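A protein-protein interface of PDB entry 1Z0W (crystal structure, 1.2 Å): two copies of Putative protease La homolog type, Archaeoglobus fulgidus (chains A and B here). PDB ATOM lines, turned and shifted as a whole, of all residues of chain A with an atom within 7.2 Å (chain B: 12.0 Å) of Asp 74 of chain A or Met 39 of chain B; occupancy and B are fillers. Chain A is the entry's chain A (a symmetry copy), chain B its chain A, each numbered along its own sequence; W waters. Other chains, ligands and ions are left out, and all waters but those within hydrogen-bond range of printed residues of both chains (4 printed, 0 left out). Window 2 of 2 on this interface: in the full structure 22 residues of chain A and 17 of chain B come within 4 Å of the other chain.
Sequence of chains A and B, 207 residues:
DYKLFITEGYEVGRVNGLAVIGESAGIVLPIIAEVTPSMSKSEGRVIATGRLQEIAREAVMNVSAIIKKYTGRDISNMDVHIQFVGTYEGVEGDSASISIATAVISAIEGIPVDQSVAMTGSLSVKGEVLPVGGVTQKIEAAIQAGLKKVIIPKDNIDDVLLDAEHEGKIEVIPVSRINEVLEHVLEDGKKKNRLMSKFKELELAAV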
ATOM      1  N   SER A  38       9.998   9.998   4.838  1.00  0.00           N
ATOM      2  CA  SER A  38       9.338  11.227   4.370  1.00  0.00           C
ATOM      3  C   SER A  38      10.321  12.405   4.310  1.00  0.00           C
ATOM      4  O   SER A  38       9.985  13.515   3.887  1.00  0.00           O
ATOM      5  CB  SER A  38       8.115  11.567   5.192  1.00  0.00           C
ATOM      6  OG  SER A  38       8.299  11.386   6.593  1.00  0.00           O
ATOM      7  N   ILE A  67      -1.345  -1.702  10.332  1.00  0.00           N
ATOM      8  CA  ILE A  67       0.108  -1.698  10.474  1.00  0.00           C
ATOM      9  C   ILE A  67       0.511  -1.023  11.783  1.00  0.00           C
ATOM     10  O   ILE A  67       1.345  -1.604  12.489  1.00  0.00           O
ATOM     11  CB  ILE A  67       0.791  -1.035   9.248  1.00  0.00           C
ATOM     12  CG1 ILE A  67       0.641  -1.971   8.021  1.00  0.00           C
ATOM     13  CG2 ILE A  67       2.225  -0.655   9.477  1.00  0.00           C
ATOM     14  CD1 ILE A  67       0.961  -1.305   6.684  1.00  0.00           C
ATOM     15  N   LYS A  68      -0.040   0.117  12.107  1.00  0.00           N
ATOM     16  CA  LYS A  68       0.320   0.819  13.354  1.00  0.00           C
ATOM     17  C   LYS A  68      -0.101  -0.034  14.548  1.00  0.00           C
ATOM     18  O   LYS A  68       0.676  -0.260  15.483  1.00  0.00           O
ATOM     19  CB  LYS A  68      -0.318   2.206  13.401  1.00  0.00           C
ATOM     20  CG  LYS A  68       0.276   3.195  12.431  1.00  0.00           C
ATOM     21  CD  LYS A  68      -0.410   4.558  12.471  1.00  0.00           C
ATOM     22  CE  LYS A  68      -1.861   4.478  12.082  1.00  0.00           C
ATOM     23  NZ  LYS A  68      -2.432   5.871  11.824  1.00  0.00           N
ATOM     24  N   LYS A  69      -1.326  -0.520  14.544  1.00  0.00           N
ATOM     25  CA  LYS A  69      -1.887  -1.182  15.690  1.00  0.00           C
ATOM     26  C   LYS A  69      -1.142  -2.486  15.984  1.00  0.00           C
ATOM     27  O   LYS A  69      -0.783  -2.709  17.150  1.00  0.00           O
ATOM     28  CB  LYS A  69      -3.389  -1.425  15.488  1.00  0.00           C
ATOM     29  CG  LYS A  69      -4.103  -2.084  16.645  1.00  0.00           C
ATOM     30  CD  LYS A  69      -5.612  -1.933  16.496  1.00  0.00           C
ATOM     31  CE  LYS A  69      -6.268  -2.785  17.573  1.00  0.00           C
ATOM     32  NZ  LYS A  69      -7.727  -2.733  17.494  1.00  0.00           N
ATOM     33  N   THR A  71       1.662  -4.060  14.099  1.00  0.00           N
ATOM     34  CA  THR A  71       3.075  -4.306  13.800  1.00  0.00           C
ATOM     35  C   THR A  71       3.972  -3.196  14.343  1.00  0.00           C
ATOM     36  O   THR A  71       5.160  -3.384  14.474  1.00  0.00           O
ATOM     37  CB  THR A  71       3.333  -4.552  12.309  1.00  0.00           C
ATOM     38  OG1 THR A  71       3.238  -3.355  11.537  1.00  0.00           O
ATOM     39  CG2 THR A  71       2.345  -5.540  11.681  1.00  0.00           C
ATOM     40  N   GLY A  72       3.435  -2.041  14.633  1.00  0.00           N
ATOM     41  CA  GLY A  72       4.155  -0.917  15.152  1.00  0.00           C
ATOM     42  C   GLY A  72       5.076  -0.233  14.187  1.00  0.00           C
ATOM     43  O   GLY A  72       5.901   0.569  14.612  1.00  0.00           O
ATOM     44  N   ARG A  73       4.998  -0.422  12.897  1.00  0.00           N
ATOM     45  CA  ARG A  73       5.768   0.291  11.900  1.00  0.00           C
ATOM     46  C   ARG A  73       5.233   1.724  11.848  1.00  0.00           C
ATOM     47  O   ARG A  73       4.025   1.947  11.829  1.00  0.00           O
ATOM     48  CB  ARG A  73       5.735  -0.304  10.516  1.00  0.00           C
ATOM     49  CG  ARG A  73       6.252  -1.696  10.272  1.00  0.00           C
ATOM     50  CD  ARG A  73       7.734  -1.699  10.014  1.00  0.00           C
ATOM     51  NE  ARG A  73       8.317  -2.985   9.706  1.00  0.00           N
ATOM     52  CZ  ARG A  73       9.178  -3.708  10.387  1.00  0.00           C
ATOM     53  NH1 ARG A  73       9.672  -3.330  11.573  1.00  0.00           N
ATOM     54  NH2 ARG A  73       9.584  -4.878   9.897  1.00  0.00           N
ATOM     55  N   ASP A  74       6.163   2.676  11.809  1.00  0.00           N
ATOM     56  CA  ASP A  74       5.793   4.094  11.823  1.00  0.00           C
ATOM     57  C   ASP A  74       5.460   4.585  10.428  1.00  0.00           C
ATOM     58  O   ASP A  74       6.159   5.383   9.843  1.00  0.00           O
ATOM     59  CB  ASP A  74       6.933   4.903  12.443  1.00  0.00           C
ATOM     60  CG  ASP A  74       6.530   6.316  12.750  1.00  0.00           C
ATOM     61  OD1 ASP A  74       5.340   6.680  12.726  1.00  0.00           O
ATOM     62  OD2 ASP A  74       7.466   7.117  13.000  1.00  0.00           O
ATOM     63  N   ILE A  75       4.334   4.095   9.900  1.00  0.00           N
ATOM     64  CA  ILE A  75       4.024   4.326   8.488  1.00  0.00           C
ATOM     65  C   ILE A  75       3.606   5.773   8.291  1.00  0.00           C
ATOM     66  O   ILE A  75       3.728   6.292   7.196  1.00  0.00           O
ATOM     67  CB  ILE A  75       2.981   3.311   8.005  1.00  0.00           C
ATOM     68  CG1 ILE A  75       2.730   3.390   6.484  1.00  0.00           C
ATOM     69  CG2 ILE A  75       1.678   3.435   8.767  1.00  0.00           C
ATOM     70  CD1 ILE A  75       1.773   2.380   5.902  1.00  0.00           C
ATOM     71  N   SER A  76       3.176   6.443   9.360  1.00  0.00           N
ATOM     72  CA  SER A  76       2.892   7.867   9.290  1.00  0.00           C
ATOM     73  C   SER A  76       4.103   8.722   8.953  1.00  0.00           C
ATOM     74  O   SER A  76       3.945   9.853   8.505  1.00  0.00           O
ATOM     75  CB  SER A  76       2.320   8.372  10.645  1.00  0.00           C
ATOM     76  OG  SER A  76       0.932   8.093  10.695  1.00  0.00           O
ATOM     77  N   ASN A  77       5.327   8.240   9.147  1.00  0.00           N
ATOM     78  CA  ASN A  77       6.559   8.927   8.784  1.00  0.00           C
ATOM     79  C   ASN A  77       7.204   8.386   7.511  1.00  0.00           C
ATOM     80  O   ASN A  77       8.395   8.575   7.230  1.00  0.00           O
ATOM     81  CB  ASN A  77       7.590   8.870   9.908  1.00  0.00           C
ATOM     82  CG  ASN A  77       7.260   9.926  10.949  1.00  0.00           C
ATOM     83  OD1 ASN A  77       6.996  11.097  10.635  1.00  0.00           O
ATOM     84  ND2 ASN A  77       7.247   9.465  12.185  1.00  0.00           N
ATOM     85  N   MET A  78       6.396   7.746   6.690  1.00  0.00           N
ATOM     86  CA  MET A  78       6.800   7.243   5.398  1.00  0.00           C
ATOM     87  C   MET A  78       6.013   7.917   4.291  1.00  0.00           C
ATOM     88  O   MET A  78       4.834   8.196   4.508  1.00  0.00           O
ATOM     89  CB  MET A  78       6.655   5.735   5.321  1.00  0.00           C
ATOM     90  CG  MET A  78       7.350   4.888   6.359  1.00  0.00           C
ATOM     91  SD  MET A  78       6.945   3.147   6.139  1.00  0.00           S
ATOM     92  CE  MET A  78       7.432   2.471   7.712  1.00  0.00           C
ATOM     93  N   ILE A 108       6.821  -2.601   2.821  1.00  0.00           N
ATOM     94  CA  ILE A 108       7.379  -2.173   4.100  1.00  0.00           C
ATOM     95  C   ILE A 108       8.192  -3.266   4.755  1.00  0.00           C
ATOM     96  O   ILE A 108       9.245  -2.958   5.371  1.00  0.00           O
ATOM     97  CB  ILE A 108       6.290  -1.666   5.018  1.00  0.00           C
ATOM     98  CG1 ILE A 108       5.721  -0.294   4.694  1.00  0.00           C
ATOM     99  CG2 ILE A 108       6.863  -1.702   6.472  1.00  0.00           C
ATOM    100  CD1 ILE A 108       4.351  -0.173   5.345  1.00  0.00           C
ATOM    101  N   GLU B  34     -11.511   2.535  13.661  1.00  0.00           N
ATOM    102  CA  GLU B  34     -10.400   1.937  14.412  1.00  0.00           C
ATOM    103  C   GLU B  34      -9.619   3.069  15.054  1.00  0.00           C
ATOM    104  O   GLU B  34      -9.507   4.154  14.521  1.00  0.00           O
ATOM    105  CB  GLU B  34      -9.529   1.073  13.509  1.00  0.00           C
ATOM    106  CG  GLU B  34      -8.354   0.397  14.243  1.00  0.00           C
ATOM    107  CD  GLU B  34      -8.824  -0.514  15.353  1.00  0.00           C
ATOM    108  OE1 GLU B  34      -9.273  -0.020  16.420  1.00  0.00           O
ATOM    109  OE2 GLU B  34      -8.752  -1.750  15.169  1.00  0.00           O
ATOM    110  N   VAL B  35      -9.059   2.787  16.235  1.00  0.00           N
ATOM    111  CA  VAL B  35      -8.201   3.740  16.926  1.00  0.00           C
ATOM    112  C   VAL B  35      -6.847   3.061  17.123  1.00  0.00           C
ATOM    113  O   VAL B  35      -6.744   1.851  17.310  1.00  0.00           O
ATOM    114  CB  VAL B  35      -8.814   4.166  18.263  1.00  0.00           C
ATOM    115  CG1 VAL B  35     -10.144   4.872  17.953  1.00  0.00           C
ATOM    116  CG2 VAL B  35      -8.947   3.030  19.245  1.00  0.00           C
ATOM    117  N   THR B  36      -5.792   3.849  16.998  1.00  0.00           N
ATOM    118  CA  THR B  36      -4.434   3.370  17.121  1.00  0.00           C
ATOM    119  C   THR B  36      -3.653   4.351  17.964  1.00  0.00           C
ATOM    120  O   THR B  36      -4.022   5.514  18.024  1.00  0.00           O
ATOM    121  CB  THR B  36      -3.673   3.185  15.770  1.00  0.00           C
ATOM    122  OG1 THR B  36      -3.252   4.431  15.226  1.00  0.00           O
ATOM    123  CG2 THR B  36      -4.619   2.580  14.738  1.00  0.00           C
ATOM    124  N   PRO B  37      -2.564   3.924  18.588  1.00  0.00           N
ATOM    125  CA  PRO B  37      -1.686   4.949  19.181  1.00  0.00           C
ATOM    126  C   PRO B  37      -1.140   5.840  18.071  1.00  0.00           C
ATOM    127  O   PRO B  37      -1.021   5.469  16.909  1.00  0.00           O
ATOM    128  CB  PRO B  37      -0.582   4.150  19.867  1.00  0.00           C
ATOM    129  CG  PRO B  37      -1.095   2.762  19.967  1.00  0.00           C
ATOM    130  CD  PRO B  37      -2.056   2.576  18.796  1.00  0.00           C
ATOM    131  N   SER B  38      -0.780   7.072  18.379  1.00  0.00           N
ATOM    132  CA  SER B  38      -0.322   7.998  17.331  1.00  0.00           C
ATOM    133  C   SER B  38       1.173   7.813  17.032  1.00  0.00           C
ATOM    134  O   SER B  38       1.745   8.451  16.142  1.00  0.00           O
ATOM    135  CB  SER B  38      -0.648   9.438  17.658  1.00  0.00           C
ATOM    136  OG  SER B  38      -0.411   9.784  19.020  1.00  0.00           O
ATOM    137  N   MET B  39       1.790   6.891  17.714  1.00  0.00           N
ATOM    138  CA  MET B  39       3.189   6.515  17.450  1.00  0.00           C
ATOM    139  C   MET B  39       4.154   7.654  17.665  1.00  0.00           C
ATOM    140  O   MET B  39       3.876   8.840  17.460  1.00  0.00           O
ATOM    141  CB  MET B  39       3.288   6.013  16.000  1.00  0.00           C
ATOM    142  CG  MET B  39       2.198   4.994  15.658  1.00  0.00           C
ATOM    143  SD  MET B  39       2.497   3.351  16.356  1.00  0.00           S
ATOM    144  CE  MET B  39       3.663   2.715  15.151  1.00  0.00           C
ATOM    145  N   GLU B  43       1.080  14.137  17.982  1.00  0.00           N
ATOM    146  CA  GLU B  43      -0.341  14.290  18.169  1.00  0.00           C
ATOM    147  C   GLU B  43      -1.137  13.356  17.265  1.00  0.00           C
ATOM    148  O   GLU B  43      -0.741  13.073  16.137  1.00  0.00           O
ATOM    149  CB  GLU B  43      -0.818  15.721  17.853  1.00  0.00           C
ATOM    150  CG  GLU B  43      -2.020  16.067  18.753  1.00  0.00           C
ATOM    151  CD  GLU B  43      -1.485  17.084  19.755  1.00  0.00           C
ATOM    152  OE1 GLU B  43      -0.452  17.684  19.372  1.00  0.00           O
ATOM    153  OE2 GLU B  43      -2.062  17.225  20.842  1.00  0.00           O
ATOM    154  N   GLY B  44      -2.275  12.878  17.732  1.00  0.00           N
ATOM    155  CA  GLY B  44      -3.071  11.949  16.921  1.00  0.00           C
ATOM    156  C   GLY B  44      -3.815  12.719  15.828  1.00  0.00           C
ATOM    157  O   GLY B  44      -4.023  13.924  15.929  1.00  0.00           O
ATOM    158  N   ARG B  45      -4.208  11.981  14.790  1.00  0.00           N
ATOM    159  CA  ARG B  45      -4.896  12.470  13.624  1.00  0.00           C
ATOM    160  C   ARG B  45      -6.289  11.857  13.445  1.00  0.00           C
ATOM    161  O   ARG B  45      -6.446  10.699  13.838  1.00  0.00           O
ATOM    162  CB  ARG B  45      -4.059  12.151  12.366  1.00  0.00           C
ATOM    163  CG  ARG B  45      -2.577  12.452  12.483  1.00  0.00           C
ATOM    164  CD  ARG B  45      -2.046  12.634  11.072  1.00  0.00           C
ATOM    165  NE  ARG B  45      -1.844  11.379  10.354  1.00  0.00           N
ATOM    166  CZ  ARG B  45      -2.078  11.137   9.066  1.00  0.00           C
ATOM    167  NH1 ARG B  45      -2.556  12.065   8.233  1.00  0.00           N
ATOM    168  NH2 ARG B  45      -1.824   9.919   8.584  1.00  0.00           N
ATOM    169  N   VAL B  46      -7.257  12.530  12.826  1.00  0.00           N
ATOM    170  CA  VAL B  46      -8.495  11.947  12.306  1.00  0.00           C
ATOM    171  C   VAL B  46      -8.166  11.601  10.863  1.00  0.00           C
ATOM    172  O   VAL B  46      -7.811  12.496  10.115  1.00  0.00           O
ATOM    173  CB  VAL B  46      -9.742  12.860  12.334  1.00  0.00           C
ATOM    174  CG1 VAL B  46     -10.927  12.085  11.736  1.00  0.00           C
ATOM    175  CG2 VAL B  46     -10.073  13.399  13.713  1.00  0.00           C
ATOM    176  N   ILE B  47      -8.220  10.333  10.527  1.00  0.00           N
ATOM    177  CA  ILE B  47      -7.842   9.812   9.224  1.00  0.00           C
ATOM    178  C   ILE B  47      -9.109   9.342   8.510  1.00  0.00           C
ATOM    179  O   ILE B  47      -9.730   8.358   8.912  1.00  0.00           O
ATOM    180  CB  ILE B  47      -6.783   8.733   9.326  1.00  0.00           C
ATOM    181  CG1 ILE B  47      -5.549   9.311  10.067  1.00  0.00           C
ATOM    182  CG2 ILE B  47      -6.356   8.125   8.006  1.00  0.00           C
ATOM    183  CD1 ILE B  47      -4.467   8.324  10.434  1.00  0.00           C
ATOM    184  N   ASP B  74      -7.440   9.201  26.628  1.00  0.00           N
ATOM    185  CA  ASP B  74      -6.570  10.197  25.999  1.00  0.00           C
ATOM    186  C   ASP B  74      -6.657  10.123  24.488  1.00  0.00           C
ATOM    187  O   ASP B  74      -5.727   9.748  23.807  1.00  0.00           O
ATOM    188  CB  ASP B  74      -5.136   9.988  26.487  1.00  0.00           C
ATOM    189  CG  ASP B  74      -4.233  11.128  26.114  1.00  0.00           C
ATOM    190  OD1 ASP B  74      -4.680  12.207  25.685  1.00  0.00           O
ATOM    191  OD2 ASP B  74      -3.000  10.918  26.230  1.00  0.00           O
ATOM    192  N   ILE B  75      -7.819  10.518  23.959  1.00  0.00           N
ATOM    193  CA  ILE B  75      -8.097  10.290  22.541  1.00  0.00           C
ATOM    194  C   ILE B  75      -7.272  11.251  21.701  1.00  0.00           C
ATOM    195  O   ILE B  75      -7.005  10.967  20.547  1.00  0.00           O
ATOM    196  CB  ILE B  75      -9.605  10.378  22.277  1.00  0.00           C
ATOM    197  CG1 ILE B  75      -9.984   9.982  20.834  1.00  0.00           C
ATOM    198  CG2 ILE B  75     -10.158  11.746  22.618  1.00  0.00           C
ATOM    199  CD1 ILE B  75     -11.455   9.967  20.499  1.00  0.00           C
ATOM    200  N   SER B  76      -6.816  12.354  22.294  1.00  0.00           N
ATOM    201  CA  SER B  76      -5.904  13.253  21.608  1.00  0.00           C
ATOM    202  C   SER B  76      -4.572  12.619  21.239  1.00  0.00           C
ATOM    203  O   SER B  76      -3.881  13.122  20.359  1.00  0.00           O
ATOM    204  CB  SER B  76      -5.606  14.498  22.489  1.00  0.00           C
ATOM    205  OG  SER B  76      -6.656  15.437  22.335  1.00  0.00           O
ATOM    206  N   ASN B  77      -4.162  11.526  21.875  1.00  0.00           N
ATOM    207  CA  ASN B  77      -2.952  10.780  21.555  1.00  0.00           C
ATOM    208  C   ASN B  77      -3.218   9.495  20.777  1.00  0.00           C
ATOM    209  O   ASN B  77      -2.400   8.566  20.716  1.00  0.00           O
ATOM    210  CB  ASN B  77      -2.156  10.429  22.809  1.00  0.00           C
ATOM    211  CG  ASN B  77      -1.346  11.636  23.248  1.00  0.00           C
ATOM    212  OD1 ASN B  77      -0.664  12.294  22.448  1.00  0.00           O
ATOM    213  ND2 ASN B  77      -1.477  11.924  24.529  1.00  0.00           N
ATOM    214  N   MET B  78      -4.357   9.453  20.117  1.00  0.00           N
ATOM    215  CA  MET B  78      -4.744   8.361  19.254  1.00  0.00           C
ATOM    216  C   MET B  78      -4.911   8.843  17.825  1.00  0.00           C
ATOM    217  O   MET B  78      -5.373   9.971  17.646  1.00  0.00           O
ATOM    218  CB  MET B  78      -6.009   7.687  19.747  1.00  0.00           C
ATOM    219  CG  MET B  78      -6.044   7.161  21.161  1.00  0.00           C
ATOM    220  SD  MET B  78      -7.674   6.507  21.560  1.00  0.00           S
ATOM    221  CE  MET B  78      -7.601   6.445  23.338  1.00  0.00           C
ATOM    222  N   ASP B  79      -4.628   7.968  16.868  1.00  0.00           N
ATOM    223  CA  ASP B  79      -5.143   8.166  15.522  1.00  0.00           C
ATOM    224  C   ASP B  79      -6.520   7.492  15.430  1.00  0.00           C
ATOM    225  O   ASP B  79      -6.689   6.378  15.860  1.00  0.00           O
ATOM    226  CB  ASP B  79      -4.184   7.614  14.477  1.00  0.00           C
ATOM    227  CG  ASP B  79      -2.896   8.389  14.320  1.00  0.00           C
ATOM    228  OD1 ASP B  79      -2.817   9.557  14.745  1.00  0.00           O
ATOM    229  OD2 ASP B  79      -1.954   7.782  13.735  1.00  0.00           O
ATOM    230  N   VAL B  80      -7.469   8.204  14.832  1.00  0.00           N
ATOM    231  CA  VAL B  80      -8.831   7.743  14.680  1.00  0.00           C
ATOM    232  C   VAL B  80      -9.127   7.600  13.185  1.00  0.00           C
ATOM    233  O   VAL B  80      -9.141   8.607  12.458  1.00  0.00           O
ATOM    234  CB  VAL B  80      -9.861   8.657  15.350  1.00  0.00           C
ATOM    235  CG1 VAL B  80     -11.256   8.056  15.156  1.00  0.00           C
ATOM    236  CG2 VAL B  80      -9.525   8.909  16.821  1.00  0.00           C
ATOM    237  N   HIS B  81      -9.292   6.364  12.756  1.00  0.00           N
ATOM    238  CA  HIS B  81      -9.578   6.023  11.365  1.00  0.00           C
ATOM    239  C   HIS B  81     -11.076   5.780  11.176  1.00  0.00           C
ATOM    240  O   HIS B  81     -11.629   4.925  11.852  1.00  0.00           O
ATOM    241  CB  HIS B  81      -8.809   4.769  10.941  1.00  0.00           C
ATOM    242  CG  HIS B  81      -7.354   4.918  10.887  1.00  0.00           C
ATOM    243  ND1 HIS B  81      -6.663   4.901   9.664  1.00  0.00           N
ATOM    244  CD2 HIS B  81      -6.377   5.078  11.777  1.00  0.00           C
ATOM    245  CE1 HIS B  81      -5.355   5.067   9.907  1.00  0.00           C
ATOM    246  NE2 HIS B  81      -5.141   5.147  11.205  1.00  0.00           N
HETATM  247  O   HOH W   1       0.693   7.780  13.763  1.00  0.00           O
HETATM  248  O   HOH W   2      -1.020   9.645  12.237  1.00  0.00           O
HETATM  249  O   HOH W   3      -7.331  -0.238  19.149  1.00  0.00           O
HETATM  250  O   HOH W   4      -1.071   6.689   9.443  1.00  0.00           O
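Positions printed for both chains: 38, 74, 75, 76, 77 and 78.
Water W2 lies within hydrogen-bond range of OD2 of Asp 79 of chain B, NE of Arg 45 of chain B and OG of Ser 76 of chain A. Water W1 lies within hydrogen-bond range of the side-chain carboxylate (OD2) of Asp 79 of chain B, the backbone carbonyl oxygen (O) of Ser 38 of chain B and the side-chain hydroxyl (OG) of Ser 76 of chain A. Water W4 lies within hydrogen-bond range of the side-chain hydroxyl (OG) of Ser 76 of chain A (2.7 Å), the side-chain amino group (NZ) of Lys 68 of chain A (2.9 Å) and the guanidinium group (NH2) of Arg 45 of chain B (3.4 Å). Water W3 lies within hydrogen-bond range of the backbone carbonyl oxygen (O) of Val 35 of chain B (2.8 Å), the side-chain amino group (NZ) of Lys 69 of chain A (3.0 Å) and the side-chain carboxylate (OE1) of Glu 34 of chain B (3.4 Å).
Printed residues of chain A that touch a printed residue of chain B: Lys 68, Lys 69, Gly 72, Arg 73, Asp 74 and Ser 76. Hydrophobic or aromatic side chains of chain B within 4 Å of the printed part of chain A: Met 39, Ile 47 and His 81. Among the printed residues, Asp or Glu carboxylates within 4 Å of a Lys or Arg side-chain nitrogen of the other chain: Lys 68 of chain A with Asp 79 of chain B and Lys 69 of chain A with Glu 34 of chain B.
The side-chain carboxylate (OE2) of Glu 34 of chain B lies within salt-bridge range of the side-chain amino group (NZ) of Lys 69 of chain A (2.7 Å). NE2 of His 81 of chain B sits at hydrogen-bond distance from NZ of Lys 68 of chain A. NZ of Lys 68 of chain A lies within salt-bridge range of OD2 of Asp 79 of chain B (2.7 Å).
Gly 72 of chain A touches one residue of chain B. Asp 74 of chain A touches one residue of chain B. No residue of chain B comes within 4 Å of Ile 75 of chain A. Of chain B, only Arg 45 (3.9 Å) comes within 4 Å of Ser 76 of chain A. Asn 77 of chain A touches none of the printed residues of chain B. Of the printed residues of chain A, Glu 34 of chain B touches Lys 69 (2.7 Å). Of the printed residues of chain A, Met 39 of chain B touches Gly 72 (3.1 Å), Arg 73 (3.4 Å) and Asp 74 (3.9 Å). Asn 77 of chain B touches none of the printed residues of chain A. Of the printed residues of chain A, His 81 of chain B touches Lys 68 (2.9 Å). The nearest residue of chain B that does not touch Asp 74 of chain A is Ser 38 of chain B (5.3 Å). The nearest residue of chain A that does not touch Met 39 of chain B is Lys 68 of chain A (4.1 Å).
The backbone carbonyl oxygen (O) of Thr 36 of chain B sits at hydrogen-bond distance from the backbone NH (N) of Asp 79 of chain B (2.8 Å). OD2 of Asp 74 of chain A is in hydrogen-bond range of ND2 of Asn 77 of chain A (2.5 Å). The backbone carbonyl oxygen (O) of Val 80 of chain B sits at hydrogen-bond distance from the backbone NH (N) of Ile 47 of chain B, 2.7 Å away. O of Glu 34 of chain B is in hydrogen-bond range of N of His 81 of chain B (2.8 Å). The backbone NH (N) of Gly 72 of chain A sits at hydrogen-bond distance from the backbone carbonyl oxygen (O) of Ile 67 of chain A, at 3.0 Å. The backbone NH (N) of Arg 45 of chain B lies within hydrogen-bond range of the side-chain carboxylate (OD1) of Asp 79 of chain B, 2.8 Å away.
Among the printed residues, merely in contact across the chains: Lys 68 of chain A with Thr 36 of chain B, Lys 68 of chain A with Ile 47 of chain B, Gly 72 of chain A with Met 39 of chain B, Arg 73 of chain A with Met 39 of chain B, Asp 74 of chain A with Met 39 of chain B and Ser 76 of chain A with Arg 45 of chain B.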
